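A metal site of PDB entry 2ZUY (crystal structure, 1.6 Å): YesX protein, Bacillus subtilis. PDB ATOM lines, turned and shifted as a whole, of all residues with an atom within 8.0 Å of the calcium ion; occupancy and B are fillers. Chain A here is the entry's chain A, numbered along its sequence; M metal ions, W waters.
Water W1 lies within hydrogen-bond range of OD1 of Asp 129 (2.6 Å) and NZ of Lys 161 (2.8 Å).
OD1 of Asp 125 lies close to N of Gly 128, 3.0 Å away. The side-chain carboxylate of Glu 133 sits close to the side-chain amino group of Lys 161, 3.1 Å away. The backbone NH (N) of Gly 130 lies within hydrogen-bond range of the side-chain carboxylate (OD2) of Asp 125 (2.8 Å). The side-chain carboxylate (OE2) of Glu 133 lies close to the backbone NH (N) of Ile 126, 2.8 Å away. O of Gly 124 sits at hydrogen-bond distance from N of Glu 133 (2.9 Å). The side-chain amino group (NZ) of Lys 161 is in salt-bridge range of the side-chain carboxylate (OD2) of Asp 127 (2.7 Å).
The calcium ion is bound by OD1 of Asp 127, OD2 of Asp 129, O of Glu 131, OD1 of Asp 125, OE1 of Glu 133, water W1 and OE2 of Glu 133. The calcium ion has seven donor atoms within binding distance.
Lys 161 touches the calcium ion. Six residues have an atom within 4 Å of the calcium ion: Asp 125, Asp 127, Asp 129, Glu 131, Glu 133 and Lys 161. The nearest printed residue that does not touch the calcium ion is Ile 126 (4.3 Å).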
ATOM      1  N   TYR A  10     -11.811  -7.792  16.295  1.00  0.00           N
ATOM      2  CA  TYR A  10     -10.793  -8.581  15.624  1.00  0.00           C
ATOM      3  C   TYR A  10      -9.909  -9.243  16.680  1.00  0.00           C
ATOM      4  O   TYR A  10      -9.431  -8.580  17.594  1.00  0.00           O
ATOM      5  CB  TYR A  10      -9.923  -7.707  14.726  1.00  0.00           C
ATOM      6  CG  TYR A  10      -8.766  -8.472  14.145  1.00  0.00           C
ATOM      7  CD1 TYR A  10      -7.457  -8.204  14.538  1.00  0.00           C
ATOM      8  CD2 TYR A  10      -8.979  -9.488  13.206  1.00  0.00           C
ATOM      9  CE1 TYR A  10      -6.396  -8.924  14.015  1.00  0.00           C
ATOM     10  CE2 TYR A  10      -7.928 -10.211  12.685  1.00  0.00           C
ATOM     11  CZ  TYR A  10      -6.631  -9.922  13.099  1.00  0.00           C
ATOM     12  OH  TYR A  10      -5.570 -10.642  12.576  1.00  0.00           O
ATOM     13  N   GLY A 124      -9.402  -4.427  26.764  1.00  0.00           N
ATOM     14  CA  GLY A 124      -9.800  -3.936  25.465  1.00  0.00           C
ATOM     15  C   GLY A 124      -8.576  -3.964  24.579  1.00  0.00           C
ATOM     16  O   GLY A 124      -7.453  -3.907  25.067  1.00  0.00           O
ATOM     17  N   ASP A 125      -8.801  -4.083  23.277  1.00  0.00           N
ATOM     18  CA  ASP A 125      -7.709  -3.997  22.320  1.00  0.00           C
ATOM     19  C   ASP A 125      -7.581  -2.530  21.931  1.00  0.00           C
ATOM     20  O   ASP A 125      -8.350  -2.018  21.121  1.00  0.00           O
ATOM     21  CB  ASP A 125      -8.010  -4.866  21.108  1.00  0.00           C
ATOM     22  CG  ASP A 125      -6.900  -4.829  20.070  1.00  0.00           C
ATOM     23  OD1 ASP A 125      -5.824  -4.248  20.330  1.00  0.00           O
ATOM     24  OD2 ASP A 125      -7.131  -5.380  18.967  1.00  0.00           O
ATOM     25  N   ILE A 126      -6.630  -1.846  22.548  1.00  0.00           N
ATOM     26  CA  ILE A 126      -6.563  -0.389  22.410  1.00  0.00           C
ATOM     27  C   ILE A 126      -5.884   0.087  21.124  1.00  0.00           C
ATOM     28  O   ILE A 126      -6.040   1.251  20.738  1.00  0.00           O
ATOM     29  CB  ILE A 126      -5.988   0.304  23.681  1.00  0.00           C
ATOM     30  CG1 ILE A 126      -4.615  -0.242  24.088  1.00  0.00           C
ATOM     31  CG2 ILE A 126      -6.937   0.095  24.855  1.00  0.00           C
ATOM     32  CD1 ILE A 126      -3.465   0.176  23.203  1.00  0.00           C
ATOM     33  N   ASP A 127      -5.183  -0.823  20.444  1.00  0.00           N
ATOM     34  CA  ASP A 127      -4.467  -0.479  19.204  1.00  0.00           C
ATOM     35  C   ASP A 127      -4.889  -1.277  17.963  1.00  0.00           C
ATOM     36  O   ASP A 127      -4.370  -1.036  16.859  1.00  0.00           O
ATOM     37  CB  ASP A 127      -2.926  -0.499  19.400  1.00  0.00           C
ATOM     38  CG  ASP A 127      -2.409  -1.782  20.033  1.00  0.00           C
ATOM     39  OD1 ASP A 127      -3.193  -2.733  20.270  1.00  0.00           O
ATOM     40  OD2 ASP A 127      -1.187  -1.835  20.285  1.00  0.00           O
ATOM     41  N   GLY A 128      -5.830  -2.202  18.141  1.00  0.00           N
ATOM     42  CA  GLY A 128      -6.472  -2.882  17.023  1.00  0.00           C
ATOM     43  C   GLY A 128      -5.689  -4.015  16.383  1.00  0.00           C
ATOM     44  O   GLY A 128      -5.948  -4.386  15.239  1.00  0.00           O
ATOM     45  N   ASP A 129      -4.747  -4.585  17.131  1.00  0.00           N
ATOM     46  CA  ASP A 129      -3.899  -5.649  16.593  1.00  0.00           C
ATOM     47  C   ASP A 129      -4.409  -7.076  16.883  1.00  0.00           C
ATOM     48  O   ASP A 129      -3.750  -8.057  16.519  1.00  0.00           O
ATOM     49  CB  ASP A 129      -2.458  -5.478  17.083  1.00  0.00           C
ATOM     50  CG  ASP A 129      -2.283  -5.846  18.550  1.00  0.00           C
ATOM     51  OD1 ASP A 129      -1.142  -6.137  18.950  1.00  0.00           O
ATOM     52  OD2 ASP A 129      -3.276  -5.829  19.306  1.00  0.00           O
ATOM     53  N   GLY A 130      -5.560  -7.163  17.552  1.00  0.00           N
ATOM     54  CA  GLY A 130      -6.174  -8.450  17.841  1.00  0.00           C
ATOM     55  C   GLY A 130      -5.700  -9.115  19.116  1.00  0.00           C
ATOM     56  O   GLY A 130      -5.952 -10.298  19.345  1.00  0.00           O
ATOM     57  N   GLU A 131      -5.020  -8.352  19.966  1.00  0.00           N
ATOM     58  CA  GLU A 131      -4.593  -8.817  21.286  1.00  0.00           C
ATOM     59  C   GLU A 131      -5.058  -7.833  22.337  1.00  0.00           C
ATOM     60  O   GLU A 131      -4.934  -6.618  22.144  1.00  0.00           O
ATOM     61  CB  GLU A 131      -3.077  -8.950  21.360  1.00  0.00           C
ATOM     62  CG  GLU A 131      -2.437  -9.757  20.221  1.00  0.00           C
ATOM     63  CD  GLU A 131      -2.674 -11.260  20.293  1.00  0.00           C
ATOM     64  OE1 GLU A 131      -2.094 -12.013  19.503  1.00  0.00           O
ATOM     65  OE2 GLU A 131      -3.522 -11.707  21.215  1.00  0.00           O
ATOM     66  N   TYR A 132      -5.573  -8.338  23.457  1.00  0.00           N
ATOM     67  CA  TYR A 132      -6.073  -7.482  24.521  1.00  0.00           C
ATOM     68  C   TYR A 132      -4.969  -6.825  25.330  1.00  0.00           C
ATOM     69  O   TYR A 132      -3.944  -7.436  25.600  1.00  0.00           O
ATOM     70  CB  TYR A 132      -6.972  -8.275  25.490  1.00  0.00           C
ATOM     71  CG  TYR A 132      -8.267  -8.722  24.871  1.00  0.00           C
ATOM     72  CD1 TYR A 132      -9.240  -7.782  24.478  1.00  0.00           C
ATOM     73  CD2 TYR A 132      -8.538 -10.075  24.675  1.00  0.00           C
ATOM     74  CE1 TYR A 132     -10.422  -8.191  23.893  1.00  0.00           C
ATOM     75  CE2 TYR A 132      -9.726 -10.491  24.099  1.00  0.00           C
ATOM     76  CZ  TYR A 132     -10.669  -9.541  23.714  1.00  0.00           C
ATOM     77  OH  TYR A 132     -11.839  -9.944  23.141  1.00  0.00           O
ATOM     78  N   GLU A 133      -5.212  -5.559  25.687  1.00  0.00           N
ATOM     79  CA  GLU A 133      -4.462  -4.862  26.734  1.00  0.00           C
ATOM     80  C   GLU A 133      -5.264  -4.935  28.035  1.00  0.00           C
ATOM     81  O   GLU A 133      -6.499  -5.119  28.008  1.00  0.00           O
ATOM     82  CB  GLU A 133      -4.234  -3.390  26.372  1.00  0.00           C
ATOM     83  CG  GLU A 133      -3.129  -3.137  25.348  1.00  0.00           C
ATOM     84  CD  GLU A 133      -3.416  -3.752  23.988  1.00  0.00           C
ATOM     85  OE1 GLU A 133      -2.592  -4.568  23.520  1.00  0.00           O
ATOM     86  OE2 GLU A 133      -4.457  -3.441  23.380  1.00  0.00           O
ATOM     87  N   MET A 134      -4.562  -4.795  29.157  1.00  0.00           N
ATOM     88  CA  MET A 134      -5.160  -4.778  30.490  1.00  0.00           C
ATOM     89  C   MET A 134      -5.425  -3.338  30.930  1.00  0.00           C
ATOM     90  O   MET A 134      -4.514  -2.509  30.890  1.00  0.00           O
ATOM     91  CB  MET A 134      -4.216  -5.418  31.511  1.00  0.00           C
ATOM     92  CG  MET A 134      -3.838  -6.879  31.231  1.00  0.00           C
ATOM     93  SD  MET A 134      -5.236  -8.003  31.181  1.00  0.00           S
ATOM     94  CE  MET A 134      -6.203  -7.422  32.578  1.00  0.00           C
ATOM     95  N   TYR A 160      -1.808  -1.549  30.377  1.00  0.00           N
ATOM     96  CA  TYR A 160      -0.627  -2.385  30.175  1.00  0.00           C
ATOM     97  C   TYR A 160      -0.793  -3.328  28.998  1.00  0.00           C
ATOM     98  O   TYR A 160      -1.881  -3.870  28.784  1.00  0.00           O
ATOM     99  CB  TYR A 160      -0.368  -3.265  31.396  1.00  0.00           C
ATOM    100  CG  TYR A 160       0.019  -2.493  32.633  1.00  0.00           C
ATOM    101  CD1 TYR A 160      -0.950  -2.105  33.554  1.00  0.00           C
ATOM    102  CD2 TYR A 160       1.350  -2.156  32.873  1.00  0.00           C
ATOM    103  CE1 TYR A 160      -0.610  -1.390  34.692  1.00  0.00           C
ATOM    104  CE2 TYR A 160       1.703  -1.443  34.016  1.00  0.00           C
ATOM    105  CZ  TYR A 160       0.706  -1.052  34.912  1.00  0.00           C
ATOM    106  OH  TYR A 160       1.035  -0.342  36.037  1.00  0.00           O
ATOM    107  N   LYS A 161       0.294  -3.551  28.262  1.00  0.00           N
ATOM    108  CA  LYS A 161       0.337  -4.635  27.288  1.00  0.00           C
ATOM    109  C   LYS A 161       0.714  -5.919  28.016  1.00  0.00           C
ATOM    110  O   LYS A 161       1.321  -5.880  29.104  1.00  0.00           O
ATOM    111  CB  LYS A 161       1.310  -4.331  26.159  1.00  0.00           C
ATOM    112  CG  LYS A 161       0.754  -3.395  25.113  1.00  0.00           C
ATOM    113  CD  LYS A 161       1.662  -3.293  23.906  1.00  0.00           C
ATOM    114  CE  LYS A 161       0.966  -2.569  22.765  1.00  0.00           C
ATOM    115  NZ  LYS A 161      -0.051  -3.428  22.101  1.00  0.00           N
ATOM    116  N   LEU A 162       0.354  -7.057  27.426  1.00  0.00           N
ATOM    117  CA  LEU A 162       0.613  -8.357  28.023  1.00  0.00           C
ATOM    118  C   LEU A 162       2.110  -8.647  28.200  1.00  0.00           C
ATOM    119  O   LEU A 162       2.477  -9.481  29.034  1.00  0.00           O
ATOM    120  CB  LEU A 162      -0.074  -9.465  27.227  1.00  0.00           C
ATOM    121  CG  LEU A 162      -1.609  -9.445  27.313  1.00  0.00           C
ATOM    122  CD1 LEU A 162      -2.224 -10.381  26.286  1.00  0.00           C
ATOM    123  CD2 LEU A 162      -2.089  -9.802  28.707  1.00  0.00           C
ATOM    124  N   LEU A 167       1.600   1.607  29.461  1.00  0.00           N
ATOM    125  CA  LEU A 167       1.181   2.522  28.382  1.00  0.00           C
ATOM    126  C   LEU A 167       0.843   3.916  28.871  1.00  0.00           C
ATOM    127  O   LEU A 167       1.318   4.904  28.320  1.00  0.00           O
ATOM    128  CB  LEU A 167       0.020   1.942  27.562  1.00  0.00           C
ATOM    129  CG  LEU A 167       0.276   0.589  26.890  1.00  0.00           C
ATOM    130  CD1 LEU A 167      -0.974   0.079  26.195  1.00  0.00           C
ATOM    131  CD2 LEU A 167       1.442   0.686  25.898  1.00  0.00           C
ATOM    132  N   GLY A 194     -12.270  -0.244  15.676  1.00  0.00           N
ATOM    133  CA  GLY A 194     -11.370  -1.357  15.937  1.00  0.00           C
ATOM    134  C   GLY A 194     -10.474  -1.189  17.168  1.00  0.00           C
ATOM    135  O   GLY A 194      -9.668  -2.078  17.484  1.00  0.00           O
HETATM  136 CA    CA M   1      -3.689  -4.751  21.350  1.00  0.00          CA
HETATM  137  O   HOH W   1      -1.391  -5.767  21.482  1.00  0.00           O
